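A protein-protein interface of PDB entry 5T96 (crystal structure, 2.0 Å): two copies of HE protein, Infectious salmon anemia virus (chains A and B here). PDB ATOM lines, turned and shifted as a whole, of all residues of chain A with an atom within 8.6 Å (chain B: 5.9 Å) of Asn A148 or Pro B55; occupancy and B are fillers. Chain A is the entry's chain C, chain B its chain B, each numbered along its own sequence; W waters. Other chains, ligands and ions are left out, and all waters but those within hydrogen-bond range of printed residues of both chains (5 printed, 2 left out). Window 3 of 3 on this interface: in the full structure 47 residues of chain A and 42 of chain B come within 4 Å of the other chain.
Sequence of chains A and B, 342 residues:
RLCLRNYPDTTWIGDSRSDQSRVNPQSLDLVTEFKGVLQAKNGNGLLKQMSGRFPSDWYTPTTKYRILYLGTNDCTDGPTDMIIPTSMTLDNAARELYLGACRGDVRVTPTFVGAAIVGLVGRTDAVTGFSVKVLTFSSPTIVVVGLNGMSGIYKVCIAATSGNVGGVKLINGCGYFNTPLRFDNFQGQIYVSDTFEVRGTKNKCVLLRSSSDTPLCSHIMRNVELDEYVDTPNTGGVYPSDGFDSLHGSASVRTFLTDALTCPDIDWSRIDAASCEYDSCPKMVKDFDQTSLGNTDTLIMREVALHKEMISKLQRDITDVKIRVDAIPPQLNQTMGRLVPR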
ATOM      1  N   ARG A 107      12.389 -35.023 -12.938  1.00  0.00           N
ATOM      2  CA  ARG A 107      13.369 -35.055 -14.027  1.00  0.00           C
ATOM      3  C   ARG A 107      14.617 -34.306 -13.601  1.00  0.00           C
ATOM      4  O   ARG A 107      14.564 -33.432 -12.730  1.00  0.00           O
ATOM      5  CB  ARG A 107      12.882 -34.386 -15.312  1.00  0.00           C
ATOM      6  CG  ARG A 107      11.640 -34.971 -15.944  1.00  0.00           C
ATOM      7  CD  ARG A 107      11.382 -34.305 -17.271  1.00  0.00           C
ATOM      8  NE  ARG A 107      12.392 -34.676 -18.269  1.00  0.00           N
ATOM      9  CZ  ARG A 107      12.722 -33.940 -19.329  1.00  0.00           C
ATOM     10  NH1 ARG A 107      12.147 -32.779 -19.539  1.00  0.00           N
ATOM     11  NH2 ARG A 107      13.652 -34.361 -20.188  1.00  0.00           N
ATOM     12  N   THR A 109      17.307 -31.888 -15.540  1.00  0.00           N
ATOM     13  CA  THR A 109      17.454 -31.216 -16.820  1.00  0.00           C
ATOM     14  C   THR A 109      18.404 -30.043 -16.680  1.00  0.00           C
ATOM     15  O   THR A 109      18.639 -29.548 -15.566  1.00  0.00           O
ATOM     16  CB  THR A 109      16.124 -30.683 -17.363  1.00  0.00           C
ATOM     17  OG1 THR A 109      15.663 -29.656 -16.461  1.00  0.00           O
ATOM     18  CG2 THR A 109      15.081 -31.820 -17.499  1.00  0.00           C
ATOM     19  N   PRO A 110      18.941 -29.553 -17.796  1.00  0.00           N
ATOM     20  CA  PRO A 110      19.859 -28.408 -17.753  1.00  0.00           C
ATOM     21  C   PRO A 110      19.161 -27.133 -17.297  1.00  0.00           C
ATOM     22  O   PRO A 110      18.061 -26.809 -17.743  1.00  0.00           O
ATOM     23  CB  PRO A 110      20.329 -28.272 -19.205  1.00  0.00           C
ATOM     24  CG  PRO A 110      20.039 -29.588 -19.862  1.00  0.00           C
ATOM     25  CD  PRO A 110      18.791 -30.097 -19.163  1.00  0.00           C
ATOM     26  N   PHE A 112      18.609 -23.160 -17.206  1.00  0.00           N
ATOM     27  CA  PHE A 112      18.891 -21.994 -18.030  1.00  0.00           C
ATOM     28  C   PHE A 112      19.826 -21.029 -17.305  1.00  0.00           C
ATOM     29  O   PHE A 112      19.658 -20.749 -16.117  1.00  0.00           O
ATOM     30  CB  PHE A 112      17.613 -21.253 -18.409  1.00  0.00           C
ATOM     31  CG  PHE A 112      17.878 -19.851 -18.909  1.00  0.00           C
ATOM     32  CD1 PHE A 112      18.405 -19.638 -20.181  1.00  0.00           C
ATOM     33  CD2 PHE A 112      17.655 -18.775 -18.088  1.00  0.00           C
ATOM     34  CE1 PHE A 112      18.681 -18.362 -20.640  1.00  0.00           C
ATOM     35  CE2 PHE A 112      17.921 -17.496 -18.519  1.00  0.00           C
ATOM     36  CZ  PHE A 112      18.440 -17.285 -19.802  1.00  0.00           C
ATOM     37  N   VAL A 145      19.457 -16.647 -14.164  1.00  0.00           N
ATOM     38  CA  VAL A 145      19.448 -18.094 -13.968  1.00  0.00           C
ATOM     39  C   VAL A 145      17.999 -18.529 -13.781  1.00  0.00           C
ATOM     40  O   VAL A 145      17.236 -17.873 -13.072  1.00  0.00           O
ATOM     41  CB  VAL A 145      20.303 -18.536 -12.761  1.00  0.00           C
ATOM     42  CG1 VAL A 145      20.394 -20.062 -12.673  1.00  0.00           C
ATOM     43  CG2 VAL A 145      21.716 -17.935 -12.820  1.00  0.00           C
ATOM     44  N   GLY A 146      17.616 -19.618 -14.444  1.00  0.00           N
ATOM     45  CA  GLY A 146      16.249 -20.102 -14.335  1.00  0.00           C
ATOM     46  C   GLY A 146      15.199 -19.310 -15.095  1.00  0.00           C
ATOM     47  O   GLY A 146      15.451 -18.221 -15.639  1.00  0.00           O
ATOM     48  N   LEU A 147      13.990 -19.864 -15.134  1.00  0.00           N
ATOM     49  CA  LEU A 147      12.897 -19.307 -15.912  1.00  0.00           C
ATOM     50  C   LEU A 147      11.618 -19.278 -15.090  1.00  0.00           C
ATOM     51  O   LEU A 147      11.349 -20.216 -14.330  1.00  0.00           O
ATOM     52  CB  LEU A 147      12.665 -20.122 -17.174  1.00  0.00           C
ATOM     53  CG  LEU A 147      13.787 -20.040 -18.213  1.00  0.00           C
ATOM     54  CD1 LEU A 147      13.599 -21.086 -19.322  1.00  0.00           C
ATOM     55  CD2 LEU A 147      13.885 -18.630 -18.798  1.00  0.00           C
ATOM     56  N   ASN A 148      10.856 -18.178 -15.240  1.00  0.00           N
ATOM     57  CA  ASN A 148       9.516 -18.063 -14.661  1.00  0.00           C
ATOM     58  C   ASN A 148       8.699 -19.292 -14.993  1.00  0.00           C
ATOM     59  O   ASN A 148       8.701 -19.772 -16.136  1.00  0.00           O
ATOM     60  CB  ASN A 148       8.772 -16.835 -15.208  1.00  0.00           C
ATOM     61  CG  ASN A 148       9.286 -15.522 -14.656  1.00  0.00           C
ATOM     62  OD1 ASN A 148       9.968 -15.478 -13.636  1.00  0.00           O
ATOM     63  ND2 ASN A 148       8.926 -14.429 -15.323  1.00  0.00           N
ATOM     64  N   GLY A 149       7.970 -19.788 -13.989  1.00  0.00           N
ATOM     65  CA  GLY A 149       7.158 -20.956 -14.146  1.00  0.00           C
ATOM     66  C   GLY A 149       7.874 -22.262 -13.869  1.00  0.00           C
ATOM     67  O   GLY A 149       7.236 -23.306 -13.872  1.00  0.00           O
ATOM     68  N   MET A 150       9.176 -22.238 -13.637  1.00  0.00           N
ATOM     69  CA  MET A 150       9.887 -23.465 -13.361  1.00  0.00           C
ATOM     70  C   MET A 150       9.351 -24.128 -12.094  1.00  0.00           C
ATOM     71  O   MET A 150       8.795 -23.489 -11.180  1.00  0.00           O
ATOM     72  CB  MET A 150      11.384 -23.184 -13.223  1.00  0.00           C
ATOM     73  CG  MET A 150      11.811 -22.381 -11.981  1.00  0.00           C
ATOM     74  SD  MET A 150      13.602 -22.059 -12.053  1.00  0.00           S
ATOM     75  CE  MET A 150      14.262 -23.751 -11.975  1.00  0.00           C
ATOM     76  N   SER A 151       9.582 -25.421 -12.021  1.00  0.00           N
ATOM     77  CA  SER A 151       9.141 -26.230 -10.879  1.00  0.00           C
ATOM     78  C   SER A 151      10.260 -27.218 -10.534  1.00  0.00           C
ATOM     79  O   SER A 151      10.250 -28.371 -10.966  1.00  0.00           O
ATOM     80  CB  SER A 151       7.846 -26.950 -11.215  1.00  0.00           C
ATOM     81  OG  SER A 151       7.330 -27.609 -10.071  1.00  0.00           O
ATOM     82  N   GLY A 152      11.171 -26.794  -9.675  1.00  0.00           N
ATOM     83  CA  GLY A 152      12.276 -27.641  -9.282  1.00  0.00           C
ATOM     84  C   GLY A 152      13.299 -26.827  -8.510  1.00  0.00           C
ATOM     85  O   GLY A 152      13.076 -25.662  -8.182  1.00  0.00           O
ATOM     86  N   ASN A 178      14.607 -22.302  -6.107  1.00  0.00           N
ATOM     87  CA  ASN A 178      13.492 -22.933  -6.791  1.00  0.00           C
ATOM     88  C   ASN A 178      12.695 -21.889  -7.564  1.00  0.00           C
ATOM     89  O   ASN A 178      11.538 -22.123  -7.939  1.00  0.00           O
ATOM     90  CB  ASN A 178      12.600 -23.701  -5.793  1.00  0.00           C
ATOM     91  CG  ASN A 178      11.916 -22.794  -4.785  1.00  0.00           C
ATOM     92  OD1 ASN A 178      12.041 -21.574  -4.830  1.00  0.00           O
ATOM     93  ND2 ASN A 178      11.193 -23.398  -3.868  1.00  0.00           N
ATOM     94  N   THR A 179      13.312 -20.752  -7.831  1.00  0.00           N
ATOM     95  CA  THR A 179      12.732 -19.675  -8.607  1.00  0.00           C
ATOM     96  C   THR A 179      13.853 -19.119  -9.469  1.00  0.00           C
ATOM     97  O   THR A 179      15.032 -19.285  -9.137  1.00  0.00           O
ATOM     98  CB  THR A 179      12.176 -18.546  -7.727  1.00  0.00           C
ATOM     99  OG1 THR A 179      13.212 -18.045  -6.861  1.00  0.00           O
ATOM    100  CG2 THR A 179      11.026 -19.016  -6.922  1.00  0.00           C
ATOM    101  N   PRO A 180      13.514 -18.392 -10.535  1.00  0.00           N
ATOM    102  CA  PRO A 180      14.553 -17.712 -11.312  1.00  0.00           C
ATOM    103  C   PRO A 180      15.247 -16.659 -10.477  1.00  0.00           C
ATOM    104  O   PRO A 180      14.674 -16.088  -9.556  1.00  0.00           O
ATOM    105  CB  PRO A 180      13.782 -17.074 -12.472  1.00  0.00           C
ATOM    106  CG  PRO A 180      12.399 -16.996 -12.030  1.00  0.00           C
ATOM    107  CD  PRO A 180      12.173 -18.156 -11.103  1.00  0.00           C
ATOM    108  N   LEU A 181      16.477 -16.350 -10.839  1.00  0.00           N
ATOM    109  CA  LEU A 181      17.173 -15.295 -10.129  1.00  0.00           C
ATOM    110  C   LEU A 181      17.850 -14.362 -11.123  1.00  0.00           C
ATOM    111  O   LEU A 181      18.049 -14.688 -12.301  1.00  0.00           O
ATOM    112  CB  LEU A 181      18.149 -15.878  -9.090  1.00  0.00           C
ATOM    113  CG  LEU A 181      19.319 -16.725  -9.498  1.00  0.00           C
ATOM    114  CD1 LEU A 181      20.362 -15.932 -10.266  1.00  0.00           C
ATOM    115  CD2 LEU A 181      19.944 -17.348  -8.263  1.00  0.00           C
ATOM    116  N   THR A 195      18.809 -28.825 -12.805  1.00  0.00           N
ATOM    117  CA  THR A 195      17.579 -28.666 -12.044  1.00  0.00           C
ATOM    118  C   THR A 195      17.006 -30.057 -11.740  1.00  0.00           C
ATOM    119  O   THR A 195      16.866 -30.896 -12.639  1.00  0.00           O
ATOM    120  CB  THR A 195      16.563 -27.830 -12.815  1.00  0.00           C
ATOM    121  OG1 THR A 195      17.054 -26.504 -12.971  1.00  0.00           O
ATOM    122  CG2 THR A 195      15.238 -27.777 -12.092  1.00  0.00           C
ATOM    123  N   GLU A 197      13.821 -31.298 -11.227  1.00  0.00           N
ATOM    124  CA  GLU A 197      12.430 -30.925 -11.481  1.00  0.00           C
ATOM    125  C   GLU A 197      11.523 -31.808 -10.662  1.00  0.00           C
ATOM    126  O   GLU A 197      11.663 -33.030 -10.659  1.00  0.00           O
ATOM    127  CB  GLU A 197      12.053 -31.085 -12.957  1.00  0.00           C
ATOM    128  CG  GLU A 197      12.840 -30.182 -13.873  1.00  0.00           C
ATOM    129  CD  GLU A 197      12.449 -30.289 -15.353  1.00  0.00           C
ATOM    130  OE1 GLU A 197      11.631 -31.166 -15.712  1.00  0.00           O
ATOM    131  OE2 GLU A 197      12.965 -29.479 -16.160  1.00  0.00           O
ATOM    132  N   ARG A 199       7.462 -32.199 -10.410  1.00  0.00           N
ATOM    133  CA  ARG A 199       6.215 -31.775 -11.024  1.00  0.00           C
ATOM    134  C   ARG A 199       5.071 -32.282 -10.152  1.00  0.00           C
ATOM    135  O   ARG A 199       4.992 -31.874  -8.997  1.00  0.00           O
ATOM    136  CB  ARG A 199       6.160 -32.242 -12.456  1.00  0.00           C
ATOM    137  CG  ARG A 199       7.295 -31.596 -13.313  1.00  0.00           C
ATOM    138  CD  ARG A 199       8.462 -32.536 -13.594  1.00  0.00           C
ATOM    139  NE  ARG A 199       7.989 -33.686 -14.389  1.00  0.00           N
ATOM    140  CZ  ARG A 199       7.887 -33.722 -15.719  1.00  0.00           C
ATOM    141  NH1 ARG A 199       8.250 -32.684 -16.463  1.00  0.00           N
ATOM    142  NH2 ARG A 199       7.418 -34.822 -16.318  1.00  0.00           N
ATOM    143  N   GLY B  52       6.953 -22.781 -23.656  1.00  0.00           N
ATOM    144  CA  GLY B  52       7.750 -22.131 -22.651  1.00  0.00           C
ATOM    145  C   GLY B  52       6.962 -21.654 -21.446  1.00  0.00           C
ATOM    146  O   GLY B  52       7.555 -21.138 -20.500  1.00  0.00           O
ATOM    147  N   ARG B  53       5.641 -21.766 -21.461  1.00  0.00           N
ATOM    148  CA  ARG B  53       4.896 -21.339 -20.290  1.00  0.00           C
ATOM    149  C   ARG B  53       5.150 -22.228 -19.077  1.00  0.00           C
ATOM    150  O   ARG B  53       5.048 -21.751 -17.941  1.00  0.00           O
ATOM    151  CB  ARG B  53       3.396 -21.299 -20.596  1.00  0.00           C
ATOM    152  CG  ARG B  53       3.028 -20.201 -21.579  1.00  0.00           C
ATOM    153  CD  ARG B  53       1.878 -19.451 -21.070  1.00  0.00           C
ATOM    154  NE  ARG B  53       1.370 -18.399 -21.955  1.00  0.00           N
ATOM    155  CZ  ARG B  53       1.340 -17.098 -21.690  1.00  0.00           C
ATOM    156  NH1 ARG B  53       1.806 -16.607 -20.555  1.00  0.00           N
ATOM    157  NH2 ARG B  53       0.798 -16.275 -22.568  1.00  0.00           N
ATOM    158  N   PHE B  54       5.473 -23.504 -19.288  1.00  0.00           N
ATOM    159  CA  PHE B  54       5.596 -24.483 -18.212  1.00  0.00           C
ATOM    160  C   PHE B  54       6.942 -25.175 -18.417  1.00  0.00           C
ATOM    161  O   PHE B  54       7.022 -26.347 -18.803  1.00  0.00           O
ATOM    162  CB  PHE B  54       4.430 -25.475 -18.202  1.00  0.00           C
ATOM    163  CG  PHE B  54       3.060 -24.832 -18.390  1.00  0.00           C
ATOM    164  CD1 PHE B  54       2.506 -24.041 -17.395  1.00  0.00           C
ATOM    165  CD2 PHE B  54       2.325 -25.064 -19.558  1.00  0.00           C
ATOM    166  CE1 PHE B  54       1.249 -23.435 -17.559  1.00  0.00           C
ATOM    167  CE2 PHE B  54       1.050 -24.464 -19.752  1.00  0.00           C
ATOM    168  CZ  PHE B  54       0.505 -23.645 -18.730  1.00  0.00           C
ATOM    169  N   PRO B  55       8.030 -24.453 -18.194  1.00  0.00           N
ATOM    170  CA  PRO B  55       9.340 -24.939 -18.669  1.00  0.00           C
ATOM    171  C   PRO B  55       9.803 -26.236 -18.008  1.00  0.00           C
ATOM    172  O   PRO B  55      10.707 -26.888 -18.541  1.00  0.00           O
ATOM    173  CB  PRO B  55      10.275 -23.767 -18.371  1.00  0.00           C
ATOM    174  CG  PRO B  55       9.577 -22.973 -17.248  1.00  0.00           C
ATOM    175  CD  PRO B  55       8.090 -23.133 -17.569  1.00  0.00           C
ATOM    176  N   SER B  56       9.236 -26.616 -16.857  1.00  0.00           N
ATOM    177  CA  SER B  56       9.595 -27.837 -16.153  1.00  0.00           C
ATOM    178  C   SER B  56       8.571 -28.958 -16.283  1.00  0.00           C
ATOM    179  O   SER B  56       8.743 -30.001 -15.641  1.00  0.00           O
ATOM    180  CB  SER B  56       9.772 -27.569 -14.648  1.00  0.00           C
ATOM    181  OG  SER B  56      10.703 -26.539 -14.315  1.00  0.00           O
ATOM    182  N   ASP B  57       7.511 -28.782 -17.072  1.00  0.00           N
ATOM    183  CA  ASP B  57       6.375 -29.697 -17.055  1.00  0.00           C
ATOM    184  C   ASP B  57       6.176 -30.389 -18.394  1.00  0.00           C
ATOM    185  O   ASP B  57       5.043 -30.691 -18.784  1.00  0.00           O
ATOM    186  CB  ASP B  57       5.096 -28.964 -16.646  1.00  0.00           C
ATOM    187  CG  ASP B  57       5.023 -28.721 -15.156  1.00  0.00           C
ATOM    188  OD1 ASP B  57       4.697 -29.664 -14.382  1.00  0.00           O
ATOM    189  OD2 ASP B  57       5.307 -27.579 -14.752  1.00  0.00           O
ATOM    190  N   TRP B  58       7.264 -30.659 -19.109  1.00  0.00           N
ATOM    191  CA  TRP B  58       7.152 -31.451 -20.316  1.00  0.00           C
ATOM    192  C   TRP B  58       6.662 -32.851 -19.972  1.00  0.00           C
ATOM    193  O   TRP B  58       7.023 -33.411 -18.934  1.00  0.00           O
ATOM    194  CB  TRP B  58       8.493 -31.573 -21.011  1.00  0.00           C
ATOM    195  CG  TRP B  58       8.978 -30.348 -21.662  1.00  0.00           C
ATOM    196  CD1 TRP B  58       9.530 -29.263 -21.050  1.00  0.00           C
ATOM    197  CD2 TRP B  58       8.955 -30.049 -23.068  1.00  0.00           C
ATOM    198  NE1 TRP B  58       9.864 -28.320 -21.983  1.00  0.00           N
ATOM    199  CE2 TRP B  58       9.533 -28.777 -23.229  1.00  0.00           C
ATOM    200  CE3 TRP B  58       8.525 -30.741 -24.204  1.00  0.00           C
ATOM    201  CZ2 TRP B  58       9.690 -28.168 -24.483  1.00  0.00           C
ATOM    202  CZ3 TRP B  58       8.704 -30.131 -25.475  1.00  0.00           C
ATOM    203  CH2 TRP B  58       9.274 -28.859 -25.587  1.00  0.00           C
ATOM    204  N   ARG B 123      17.147 -14.204 -21.506  1.00  0.00           N
ATOM    205  CA  ARG B 123      15.732 -14.535 -21.431  1.00  0.00           C
ATOM    206  C   ARG B 123      14.937 -13.258 -21.621  1.00  0.00           C
ATOM    207  O   ARG B 123      15.391 -12.178 -21.258  1.00  0.00           O
ATOM    208  CB  ARG B 123      15.351 -15.211 -20.084  1.00  0.00           C
ATOM    209  CG  ARG B 123      15.517 -14.328 -18.885  1.00  0.00           C
ATOM    210  CD  ARG B 123      15.252 -15.033 -17.566  1.00  0.00           C
ATOM    211  NE  ARG B 123      15.302 -14.039 -16.498  1.00  0.00           N
ATOM    212  CZ  ARG B 123      15.607 -14.278 -15.230  1.00  0.00           C
ATOM    213  NH1 ARG B 123      15.902 -15.509 -14.804  1.00  0.00           N
ATOM    214  NH2 ARG B 123      15.608 -13.268 -14.381  1.00  0.00           N
ATOM    215  N   SER B 131       8.352 -15.103 -20.282  1.00  0.00           N
ATOM    216  CA  SER B 131       9.802 -15.228 -20.226  1.00  0.00           C
ATOM    217  C   SER B 131      10.260 -16.563 -20.783  1.00  0.00           C
ATOM    218  O   SER B 131       9.888 -17.624 -20.274  1.00  0.00           O
ATOM    219  CB  SER B 131      10.277 -15.055 -18.791  1.00  0.00           C
ATOM    220  OG  SER B 131      11.684 -15.105 -18.723  1.00  0.00           O
HETATM  221  O   HOH W   1      13.221 -26.869 -15.318  1.00  0.00           O
HETATM  222  O   HOH W   2       7.970 -18.012 -18.208  1.00  0.00           O
HETATM  223  O   HOH W   3      12.426 -28.990 -18.710  1.00  0.00           O
HETATM  224  O   HOH W   4       7.071 -14.540 -17.608  1.00  0.00           O
HETATM  225  O   HOH W   5      12.295 -15.863 -16.015  1.00  0.00           O
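The backbone NH (N) of Glu A197 lies within hydrogen-bond range of the backbone carbonyl oxygen (O) of Arg A107 (2.7 Å).
The side-chain hydroxyl of Thr A109 sits at hydrogen-bond distance from the side-chain carboxylate of Glu A197 (2.7 Å).
O of Phe A112 sits at hydrogen-bond distance from N of Gly A146, 2.9 Å away.
The backbone carbonyl oxygen (O) of Val A145 sits at hydrogen-bond distance from the backbone NH (N) of Leu A181 (2.8 Å).
The guanidinium group (NH1) of Arg A199 is in salt-bridge range of the side-chain carboxylate (OE1) of Glu A197 (3.8 Å).
The side-chain hydroxyl of Ser B56 is in hydrogen-bond range of the backbone NH of Ser A151 (2.8 Å).
The backbone carbonyl oxygen of Ser B56 sits at hydrogen-bond distance from the guanidinium group of Arg A199 (2.8 Å).
O of Trp B58 sits at hydrogen-bond distance from NH1 of Arg A199 (2.9 Å).
The backbone carbonyl oxygen (O) of Val A145 lies within hydrogen-bond range of the guanidinium group (NH1) of Arg B123, 3.2 Å away.
The guanidinium group of Arg B123 lies within hydrogen-bond range of the backbone carbonyl oxygen of Gly A146 (2.9 Å).
The guanidinium group (NH1) of Arg B123 is in hydrogen-bond range of the backbone carbonyl oxygen (O) of Leu A181, 3.4 Å away.
OE1 of Glu A197 sits close to O of Ser B56.
Hydrophobic or aromatic side chains of chain B that line the printed part of chain A: Pro B55.
Along chain B the printed residues that touch a printed residue of chain A span positions 55 to 131.
Of the 19 printed residues of chain A, 12 touch a printed residue of chain B.
Hydrophobic or aromatic side chains of chain A within 4 Å of the printed part of chain B: Phe A112, Leu A147, Met A150 and Pro A180.
Among the printed residues, 16 pairs touch across the chains.
Among the printed residues, no Asp or Glu carboxylate lies within 4 Å of a Lys or Arg side-chain nitrogen of the other chain.
No position is printed for both chains.
Of the 16 pairs that touch across the chains among the printed residues, none has its exchanged pair printed and touching as well.
Phe A112 touches Arg B123 (CZ to CB, 3.7 Å).
Leu A147 touches Arg B123.
Pro B55 touches Asn A148.
Asn A148 touches Ser B131.
Pro B55 touches Gly A149 (CD to O, 3.8 Å).
N of Met A150 touches CG of Pro B55, 3.7 Å away.
Ser B56 touches Met A150 (OG to CA, 3.3 Å).
CB of Pro A180 touches NH1 of Arg B123, 3.5 Å away.
OD1 of Asp B57 touches CG of Arg A199, 3.4 Å away.
Water W3 lies within hydrogen-bond range of the side-chain carboxylate (OE2) of Glu A197 (2.7 Å) and the backbone carbonyl oxygen (O) of Pro B55 (2.7 Å).
Water W1 lies within hydrogen-bond range of OG of Ser B56 (2.7 Å) and OE2 of Glu A197 (2.8 Å).
Water W2 bridges the backbone carbonyl oxygen (O) of Asn A148 and the backbone carbonyl oxygen (O) of Ser B131.
Water W5 bridges the backbone NH (N) of Asn A148 and the side-chain hydroxyl (OG) of Ser B131.
Water W4 lies within hydrogen-bond range of the side-chain amide nitrogen of Asn A148 (2.9 Å) and the backbone NH of Ser B131 (3.0 Å).
Of the printed residues of chain A, Pro B55 touches Asn A148, Gly A149 and Met A150.
Printed residues of chain B within 4 Å of Glu A197: Ser B56.
Printed residues of chain B within 4 Å of Leu A147: Arg B123 (3.9 Å).
Of the printed residues of chain B, Phe A112 touches Arg B123.
Of the printed residues of chain A, Ser B131 touches Asn A148.
Of the printed residues of chain B, Gly A149 touches Pro B55.
The nearest residue of chain B that does not touch Asn A148 is Arg B53 (4.5 Å).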
